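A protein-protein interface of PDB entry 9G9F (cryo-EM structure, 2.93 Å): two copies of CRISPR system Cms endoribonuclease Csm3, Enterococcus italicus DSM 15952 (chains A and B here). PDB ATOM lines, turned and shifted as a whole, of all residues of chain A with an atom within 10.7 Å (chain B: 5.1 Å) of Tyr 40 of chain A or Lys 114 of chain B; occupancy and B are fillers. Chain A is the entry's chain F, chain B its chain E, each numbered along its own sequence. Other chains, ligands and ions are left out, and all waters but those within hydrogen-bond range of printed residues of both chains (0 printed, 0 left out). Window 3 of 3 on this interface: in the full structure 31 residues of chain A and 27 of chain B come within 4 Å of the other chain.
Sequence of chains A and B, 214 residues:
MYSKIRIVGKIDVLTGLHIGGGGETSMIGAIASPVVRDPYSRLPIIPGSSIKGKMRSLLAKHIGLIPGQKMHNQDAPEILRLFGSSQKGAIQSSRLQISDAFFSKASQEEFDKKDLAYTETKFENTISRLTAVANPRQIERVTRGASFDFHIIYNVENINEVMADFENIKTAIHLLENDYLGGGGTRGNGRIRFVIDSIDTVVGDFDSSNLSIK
NE of Arg 144 of chain B is in salt-bridge range of OD2 of Asp 38 of chain A, 3.0 Å away. The side-chain amino group (NZ) of Lys 114 of chain B is in hydrogen-bond range of the backbone carbonyl oxygen (O) of Tyr 40 of chain A.
The backbone NH (N) of Tyr 40 of chain A lies close to the side-chain carboxylate (OD1) of Asp 38 of chain A (3.4 Å). OD2 of Asp 38 of chain A lies within hydrogen-bond range of N of Ser 41 of chain A (3.4 Å). O of Leu 43 of chain A lies within hydrogen-bond range of N of Asp 38 of chain A, at 3.0 Å. The backbone NH (N) of Leu 116 of chain B lies within hydrogen-bond range of the backbone carbonyl oxygen (O) of Phe 111 of chain B, at 3.0 Å.
Pro 39 of chain A touches Leu 116 of chain B. Tyr 40 of chain A touches Leu 116 of chain B (CA to CD2, 3.6 Å). Gly 145 of chain B touches Tyr 40 of chain A (CA to CD2, 3.5 Å). Arg 42 of chain A touches Lys 114 of chain B. NH2 of Arg 42 of chain A touches CD1 of Leu 116 of chain B, at 3.7 Å. CE1 of Phe 102 of chain A touches CD of Arg 144 of chain B (3.4 Å).
Of the printed residues of chain B, Pro 39 of chain A touches Leu 116 (3.2 Å). Printed residues of chain B within 4 Å of Phe 102 of chain A: Arg 144. No residue of chain A comes within 4 Å of Asp 115 of chain B. The nearest printed residue of chain A that does not touch Lys 114 of chain B is Ser 41 of chain A (4.8 Å). The nearest printed residue of chain B that does not touch Asp 38 of chain A is Gly 145 of chain B (6.1 Å).
Hydrophobic or aromatic side chains of chain B that line the printed part of chain A: Leu 116. Among the printed residues, Asp or Glu carboxylates within 4 Å of a Lys or Arg side-chain nitrogen of the other chain: Asp 38 of chain A with Arg 144 of chain B.
No position is printed for both chains. Of the 8 pairs that touch across the chains among the printed residues, none has its exchanged pair printed and touching as well.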
ATOM      1  N   GLU A  24     -12.377  -1.517 -15.298  1.00  0.00           N
ATOM      2  CA  GLU A  24     -13.522  -1.938 -14.499  1.00  0.00           C
ATOM      3  C   GLU A  24     -14.117  -3.195 -15.114  1.00  0.00           C
ATOM      4  O   GLU A  24     -14.422  -3.220 -16.312  1.00  0.00           O
ATOM      5  CB  GLU A  24     -14.573  -0.829 -14.419  1.00  0.00           C
ATOM      6  CG  GLU A  24     -14.078   0.440 -13.749  1.00  0.00           C
ATOM      7  CD  GLU A  24     -13.812   0.251 -12.267  1.00  0.00           C
ATOM      8  OE1 GLU A  24     -14.434  -0.648 -11.660  1.00  0.00           O
ATOM      9  OE2 GLU A  24     -12.981   0.998 -11.710  1.00  0.00           O
ATOM     10  N   VAL A  36     -16.133   7.836 -16.118  1.00  0.00           N
ATOM     11  CA  VAL A  36     -15.132   8.053 -15.090  1.00  0.00           C
ATOM     12  C   VAL A  36     -15.834   8.358 -13.781  1.00  0.00           C
ATOM     13  O   VAL A  36     -16.903   8.980 -13.747  1.00  0.00           O
ATOM     14  CB  VAL A  36     -14.165   9.187 -15.463  1.00  0.00           C
ATOM     15  CG1 VAL A  36     -13.249   8.756 -16.579  1.00  0.00           C
ATOM     16  CG2 VAL A  36     -14.935  10.412 -15.867  1.00  0.00           C
ATOM     17  N   ARG A  37     -15.237   7.905 -12.691  1.00  0.00           N
ATOM     18  CA  ARG A  37     -15.810   8.091 -11.373  1.00  0.00           C
ATOM     19  C   ARG A  37     -14.721   8.566 -10.432  1.00  0.00           C
ATOM     20  O   ARG A  37     -13.569   8.138 -10.527  1.00  0.00           O
ATOM     21  CB  ARG A  37     -16.421   6.791 -10.842  1.00  0.00           C
ATOM     22  CG  ARG A  37     -17.601   6.269 -11.640  1.00  0.00           C
ATOM     23  CD  ARG A  37     -18.903   6.881 -11.174  1.00  0.00           C
ATOM     24  NE  ARG A  37     -20.056   6.164 -11.702  1.00  0.00           N
ATOM     25  CZ  ARG A  37     -20.481   4.997 -11.239  1.00  0.00           C
ATOM     26  NH1 ARG A  37     -19.852   4.371 -10.258  1.00  0.00           N
ATOM     27  NH2 ARG A  37     -21.566   4.444 -11.772  1.00  0.00           N
ATOM     28  N   ASP A  38     -15.088   9.456  -9.534  1.00  0.00           N
ATOM     29  CA  ASP A  38     -14.245   9.697  -8.383  1.00  0.00           C
ATOM     30  C   ASP A  38     -14.318   8.453  -7.512  1.00  0.00           C
ATOM     31  O   ASP A  38     -15.412   8.090  -7.070  1.00  0.00           O
ATOM     32  CB  ASP A  38     -14.718  10.924  -7.620  1.00  0.00           C
ATOM     33  CG  ASP A  38     -13.969  11.128  -6.325  1.00  0.00           C
ATOM     34  OD1 ASP A  38     -12.822  10.649  -6.216  1.00  0.00           O
ATOM     35  OD2 ASP A  38     -14.531  11.764  -5.411  1.00  0.00           O
ATOM     36  N   PRO A  39     -13.208   7.758  -7.262  1.00  0.00           N
ATOM     37  CA  PRO A  39     -13.298   6.515  -6.483  1.00  0.00           C
ATOM     38  C   PRO A  39     -13.860   6.718  -5.090  1.00  0.00           C
ATOM     39  O   PRO A  39     -14.523   5.816  -4.562  1.00  0.00           O
ATOM     40  CB  PRO A  39     -11.846   6.023  -6.446  1.00  0.00           C
ATOM     41  CG  PRO A  39     -11.212   6.644  -7.633  1.00  0.00           C
ATOM     42  CD  PRO A  39     -11.849   7.991  -7.767  1.00  0.00           C
ATOM     43  N   TYR A  40     -13.630   7.879  -4.479  1.00  0.00           N
ATOM     44  CA  TYR A  40     -14.122   8.116  -3.127  1.00  0.00           C
ATOM     45  C   TYR A  40     -15.637   8.275  -3.119  1.00  0.00           C
ATOM     46  O   TYR A  40     -16.357   7.474  -2.513  1.00  0.00           O
ATOM     47  CB  TYR A  40     -13.436   9.350  -2.538  1.00  0.00           C
ATOM     48  CG  TYR A  40     -13.616   9.508  -1.046  1.00  0.00           C
ATOM     49  CD1 TYR A  40     -14.776  10.055  -0.522  1.00  0.00           C
ATOM     50  CD2 TYR A  40     -12.617   9.130  -0.166  1.00  0.00           C
ATOM     51  CE1 TYR A  40     -14.941  10.205   0.837  1.00  0.00           C
ATOM     52  CE2 TYR A  40     -12.773   9.277   1.192  1.00  0.00           C
ATOM     53  CZ  TYR A  40     -13.936   9.817   1.688  1.00  0.00           C
ATOM     54  OH  TYR A  40     -14.099   9.969   3.044  1.00  0.00           O
ATOM     55  N   SER A  41     -16.140   9.300  -3.804  1.00  0.00           N
ATOM     56  CA  SER A  41     -17.571   9.572  -3.824  1.00  0.00           C
ATOM     57  C   SER A  41     -18.350   8.564  -4.656  1.00  0.00           C
ATOM     58  O   SER A  41     -19.574   8.477  -4.508  1.00  0.00           O
ATOM     59  CB  SER A  41     -17.821  10.984  -4.358  1.00  0.00           C
ATOM     60  OG  SER A  41     -19.205  11.234  -4.514  1.00  0.00           O
ATOM     61  N   ARG A  42     -17.669   7.803  -5.514  1.00  0.00           N
ATOM     62  CA  ARG A  42     -18.311   6.871  -6.438  1.00  0.00           C
ATOM     63  C   ARG A  42     -19.374   7.580  -7.270  1.00  0.00           C
ATOM     64  O   ARG A  42     -20.458   7.053  -7.517  1.00  0.00           O
ATOM     65  CB  ARG A  42     -18.899   5.672  -5.696  1.00  0.00           C
ATOM     66  CG  ARG A  42     -18.926   4.395  -6.513  1.00  0.00           C
ATOM     67  CD  ARG A  42     -19.072   3.176  -5.622  1.00  0.00           C
ATOM     68  NE  ARG A  42     -18.084   3.168  -4.551  1.00  0.00           N
ATOM     69  CZ  ARG A  42     -16.838   2.733  -4.681  1.00  0.00           C
ATOM     70  NH1 ARG A  42     -16.388   2.262  -5.832  1.00  0.00           N
ATOM     71  NH2 ARG A  42     -16.024   2.772  -3.631  1.00  0.00           N
ATOM     72  N   LEU A  43     -19.051   8.792  -7.704  1.00  0.00           N
ATOM     73  CA  LEU A  43     -19.952   9.654  -8.451  1.00  0.00           C
ATOM     74  C   LEU A  43     -19.272  10.105  -9.733  1.00  0.00           C
ATOM     75  O   LEU A  43     -18.042  10.146  -9.803  1.00  0.00           O
ATOM     76  CB  LEU A  43     -20.354  10.885  -7.621  1.00  0.00           C
ATOM     77  CG  LEU A  43     -21.756  10.916  -7.008  1.00  0.00           C
ATOM     78  CD1 LEU A  43     -22.046   9.632  -6.259  1.00  0.00           C
ATOM     79  CD2 LEU A  43     -21.903  12.096  -6.076  1.00  0.00           C
ATOM     80  N   PRO A  44     -20.045  10.439 -10.764  1.00  0.00           N
ATOM     81  CA  PRO A  44     -19.436  10.915 -12.008  1.00  0.00           C
ATOM     82  C   PRO A  44     -18.667  12.206 -11.783  1.00  0.00           C
ATOM     83  O   PRO A  44     -18.978  12.994 -10.889  1.00  0.00           O
ATOM     84  CB  PRO A  44     -20.636  11.128 -12.936  1.00  0.00           C
ATOM     85  CG  PRO A  44     -21.814  11.208 -12.037  1.00  0.00           C
ATOM     86  CD  PRO A  44     -21.505  10.315 -10.883  1.00  0.00           C
ATOM     87  N   ILE A  45     -17.637  12.404 -12.598  1.00  0.00           N
ATOM     88  CA  ILE A  45     -16.717  13.521 -12.430  1.00  0.00           C
ATOM     89  C   ILE A  45     -16.236  13.959 -13.803  1.00  0.00           C
ATOM     90  O   ILE A  45     -15.990  13.127 -14.679  1.00  0.00           O
ATOM     91  CB  ILE A  45     -15.540  13.131 -11.510  1.00  0.00           C
ATOM     92  CG1 ILE A  45     -14.457  14.201 -11.509  1.00  0.00           C
ATOM     93  CG2 ILE A  45     -14.947  11.806 -11.935  1.00  0.00           C
ATOM     94  CD1 ILE A  45     -13.242  13.800 -10.722  1.00  0.00           C
ATOM     95  N   ASP A 100     -10.539  19.131 -11.302  1.00  0.00           N
ATOM     96  CA  ASP A 100     -11.655  18.210 -11.464  1.00  0.00           C
ATOM     97  C   ASP A 100     -12.965  18.866 -11.051  1.00  0.00           C
ATOM     98  O   ASP A 100     -13.014  19.658 -10.106  1.00  0.00           O
ATOM     99  CB  ASP A 100     -11.420  16.944 -10.640  1.00  0.00           C
ATOM    100  CG  ASP A 100     -10.152  16.203 -11.041  1.00  0.00           C
ATOM    101  OD1 ASP A 100      -9.071  16.822 -11.083  1.00  0.00           O
ATOM    102  OD2 ASP A 100     -10.233  14.988 -11.305  1.00  0.00           O
ATOM    103  N   PHE A 102     -16.376  18.191  -9.485  1.00  0.00           N
ATOM    104  CA  PHE A 102     -17.026  17.179  -8.672  1.00  0.00           C
ATOM    105  C   PHE A 102     -18.536  17.377  -8.650  1.00  0.00           C
ATOM    106  O   PHE A 102     -19.056  18.444  -8.979  1.00  0.00           O
ATOM    107  CB  PHE A 102     -16.491  17.210  -7.247  1.00  0.00           C
ATOM    108  CG  PHE A 102     -15.007  17.159  -7.168  1.00  0.00           C
ATOM    109  CD1 PHE A 102     -14.323  16.042  -7.595  1.00  0.00           C
ATOM    110  CD2 PHE A 102     -14.293  18.233  -6.673  1.00  0.00           C
ATOM    111  CE1 PHE A 102     -12.959  15.996  -7.529  1.00  0.00           C
ATOM    112  CE2 PHE A 102     -12.928  18.190  -6.603  1.00  0.00           C
ATOM    113  CZ  PHE A 102     -12.260  17.073  -7.033  1.00  0.00           C
ATOM    114  N   PHE A 103     -19.235  16.326  -8.236  1.00  0.00           N
ATOM    115  CA  PHE A 103     -20.689  16.341  -8.156  1.00  0.00           C
ATOM    116  C   PHE A 103     -21.127  17.218  -6.990  1.00  0.00           C
ATOM    117  O   PHE A 103     -20.723  16.986  -5.847  1.00  0.00           O
ATOM    118  CB  PHE A 103     -21.215  14.920  -7.995  1.00  0.00           C
ATOM    119  CG  PHE A 103     -22.550  14.687  -8.633  1.00  0.00           C
ATOM    120  CD1 PHE A 103     -22.645  14.406  -9.983  1.00  0.00           C
ATOM    121  CD2 PHE A 103     -23.707  14.734  -7.882  1.00  0.00           C
ATOM    122  CE1 PHE A 103     -23.864  14.185 -10.568  1.00  0.00           C
ATOM    123  CE2 PHE A 103     -24.930  14.514  -8.464  1.00  0.00           C
ATOM    124  CZ  PHE A 103     -25.009  14.238  -9.808  1.00  0.00           C
ATOM    125  N   LYS A 105     -23.397  19.116  -4.080  1.00  0.00           N
ATOM    126  CA  LYS A 105     -24.380  18.657  -3.109  1.00  0.00           C
ATOM    127  C   LYS A 105     -25.789  19.084  -3.493  1.00  0.00           C
ATOM    128  O   LYS A 105     -26.752  18.381  -3.173  1.00  0.00           O
ATOM    129  CB  LYS A 105     -24.032  19.176  -1.715  1.00  0.00           C
ATOM    130  CG  LYS A 105     -22.781  18.553  -1.120  1.00  0.00           C
ATOM    131  CD  LYS A 105     -22.437  19.178   0.222  1.00  0.00           C
ATOM    132  CE  LYS A 105     -21.174  18.568   0.806  1.00  0.00           C
ATOM    133  NZ  LYS A 105     -20.794  19.200   2.100  1.00  0.00           N
ATOM    134  N   GLN A 108     -26.947  16.643  -6.244  1.00  0.00           N
ATOM    135  CA  GLN A 108     -27.021  15.323  -5.628  1.00  0.00           C
ATOM    136  C   GLN A 108     -28.247  15.205  -4.734  1.00  0.00           C
ATOM    137  O   GLN A 108     -28.953  14.191  -4.767  1.00  0.00           O
ATOM    138  CB  GLN A 108     -25.746  15.044  -4.835  1.00  0.00           C
ATOM    139  CG  GLN A 108     -25.717  13.691  -4.160  1.00  0.00           C
ATOM    140  CD  GLN A 108     -24.418  13.441  -3.427  1.00  0.00           C
ATOM    141  OE1 GLN A 108     -23.519  14.281  -3.433  1.00  0.00           O
ATOM    142  NE2 GLN A 108     -24.313  12.283  -2.787  1.00  0.00           N
ATOM    143  N   GLU B 110      -9.976   4.581   6.292  1.00  0.00           N
ATOM    144  CA  GLU B 110     -11.149   4.936   5.498  1.00  0.00           C
ATOM    145  C   GLU B 110     -11.067   4.428   4.064  1.00  0.00           C
ATOM    146  O   GLU B 110     -12.083   4.437   3.363  1.00  0.00           O
ATOM    147  CB  GLU B 110     -11.403   6.445   5.481  1.00  0.00           C
ATOM    148  CG  GLU B 110     -12.138   6.981   6.708  1.00  0.00           C
ATOM    149  CD  GLU B 110     -11.232   7.385   7.845  1.00  0.00           C
ATOM    150  OE1 GLU B 110     -11.563   7.084   9.011  1.00  0.00           O
ATOM    151  OE2 GLU B 110     -10.235   8.081   7.580  1.00  0.00           O
ATOM    152  N   PHE B 111      -9.892   4.011   3.601  1.00  0.00           N
ATOM    153  CA  PHE B 111      -9.812   3.386   2.285  1.00  0.00           C
ATOM    154  C   PHE B 111      -9.908   1.871   2.352  1.00  0.00           C
ATOM    155  O   PHE B 111     -10.381   1.247   1.396  1.00  0.00           O
ATOM    156  CB  PHE B 111      -8.522   3.800   1.579  1.00  0.00           C
ATOM    157  CG  PHE B 111      -8.641   5.089   0.830  1.00  0.00           C
ATOM    158  CD1 PHE B 111      -9.204   5.119  -0.426  1.00  0.00           C
ATOM    159  CD2 PHE B 111      -8.208   6.271   1.389  1.00  0.00           C
ATOM    160  CE1 PHE B 111      -9.323   6.301  -1.108  1.00  0.00           C
ATOM    161  CE2 PHE B 111      -8.325   7.453   0.712  1.00  0.00           C
ATOM    162  CZ  PHE B 111      -8.883   7.469  -0.538  1.00  0.00           C
ATOM    163  N   ASP B 112      -9.459   1.261   3.452  1.00  0.00           N
ATOM    164  CA  ASP B 112      -9.742  -0.150   3.680  1.00  0.00           C
ATOM    165  C   ASP B 112     -11.235  -0.379   3.853  1.00  0.00           C
ATOM    166  O   ASP B 112     -11.779  -1.367   3.347  1.00  0.00           O
ATOM    167  CB  ASP B 112      -8.968  -0.651   4.895  1.00  0.00           C
ATOM    168  CG  ASP B 112      -7.505  -0.860   4.596  1.00  0.00           C
ATOM    169  OD1 ASP B 112      -7.111  -0.643   3.434  1.00  0.00           O
ATOM    170  OD2 ASP B 112      -6.752  -1.239   5.515  1.00  0.00           O
ATOM    171  N   LYS B 113     -11.910   0.511   4.574  1.00  0.00           N
ATOM    172  CA  LYS B 113     -13.356   0.592   4.459  1.00  0.00           C
ATOM    173  C   LYS B 113     -13.721   1.140   3.084  1.00  0.00           C
ATOM    174  O   LYS B 113     -12.934   1.835   2.438  1.00  0.00           O
ATOM    175  CB  LYS B 113     -13.944   1.473   5.561  1.00  0.00           C
ATOM    176  CG  LYS B 113     -14.035   0.791   6.914  1.00  0.00           C
ATOM    177  CD  LYS B 113     -15.009   1.511   7.832  1.00  0.00           C
ATOM    178  CE  LYS B 113     -14.390   2.761   8.430  1.00  0.00           C
ATOM    179  NZ  LYS B 113     -13.369   2.432   9.462  1.00  0.00           N
ATOM    180  N   LYS B 114     -14.924   0.801   2.630  1.00  0.00           N
ATOM    181  CA  LYS B 114     -15.432   1.079   1.290  1.00  0.00           C
ATOM    182  C   LYS B 114     -14.711   0.270   0.221  1.00  0.00           C
ATOM    183  O   LYS B 114     -15.063   0.388  -0.959  1.00  0.00           O
ATOM    184  CB  LYS B 114     -15.355   2.566   0.914  1.00  0.00           C
ATOM    185  CG  LYS B 114     -15.868   3.512   1.982  1.00  0.00           C
ATOM    186  CD  LYS B 114     -15.338   4.918   1.767  1.00  0.00           C
ATOM    187  CE  LYS B 114     -15.652   5.409   0.368  1.00  0.00           C
ATOM    188  NZ  LYS B 114     -15.089   6.761   0.118  1.00  0.00           N
ATOM    189  N   ASP B 115     -13.721  -0.547   0.589  1.00  0.00           N
ATOM    190  CA  ASP B 115     -12.985  -1.391  -0.350  1.00  0.00           C
ATOM    191  C   ASP B 115     -12.454  -0.573  -1.523  1.00  0.00           C
ATOM    192  O   ASP B 115     -12.742  -0.844  -2.690  1.00  0.00           O
ATOM    193  CB  ASP B 115     -13.850  -2.553  -0.836  1.00  0.00           C
ATOM    194  CG  ASP B 115     -13.522  -3.853  -0.137  1.00  0.00           C
ATOM    195  OD1 ASP B 115     -12.325  -4.201  -0.064  1.00  0.00           O
ATOM    196  OD2 ASP B 115     -14.458  -4.526   0.340  1.00  0.00           O
ATOM    197  N   LEU B 116     -11.668   0.447  -1.197  1.00  0.00           N
ATOM    198  CA  LEU B 116     -11.172   1.406  -2.172  1.00  0.00           C
ATOM    199  C   LEU B 116      -9.658   1.305  -2.258  1.00  0.00           C
ATOM    200  O   LEU B 116      -8.973   1.311  -1.230  1.00  0.00           O
ATOM    201  CB  LEU B 116     -11.588   2.824  -1.793  1.00  0.00           C
ATOM    202  CG  LEU B 116     -11.635   3.854  -2.916  1.00  0.00           C
ATOM    203  CD1 LEU B 116     -12.392   3.295  -4.099  1.00  0.00           C
ATOM    204  CD2 LEU B 116     -12.295   5.110  -2.410  1.00  0.00           C
ATOM    205  N   ARG B 144      -8.999  10.957  -3.811  1.00  0.00           N
ATOM    206  CA  ARG B 144      -9.337  12.219  -3.160  1.00  0.00           C
ATOM    207  C   ARG B 144      -9.304  12.129  -1.642  1.00  0.00           C
ATOM    208  O   ARG B 144      -9.055  13.136  -0.971  1.00  0.00           O
ATOM    209  CB  ARG B 144     -10.718  12.673  -3.609  1.00  0.00           C
ATOM    210  CG  ARG B 144     -10.713  13.491  -4.867  1.00  0.00           C
ATOM    211  CD  ARG B 144     -11.658  14.657  -4.726  1.00  0.00           C
ATOM    212  NE  ARG B 144     -13.029  14.237  -4.476  1.00  0.00           N
ATOM    213  CZ  ARG B 144     -13.735  14.593  -3.413  1.00  0.00           C
ATOM    214  NH1 ARG B 144     -13.229  15.385  -2.482  1.00  0.00           N
ATOM    215  NH2 ARG B 144     -14.982  14.150  -3.283  1.00  0.00           N
ATOM    216  N   GLY B 145      -9.580  10.965  -1.078  1.00  0.00           N
ATOM    217  CA  GLY B 145      -9.637  10.877   0.364  1.00  0.00           C
ATOM    218  C   GLY B 145      -8.305  10.783   1.059  1.00  0.00           C
ATOM    219  O   GLY B 145      -8.259  10.699   2.288  1.00  0.00           O
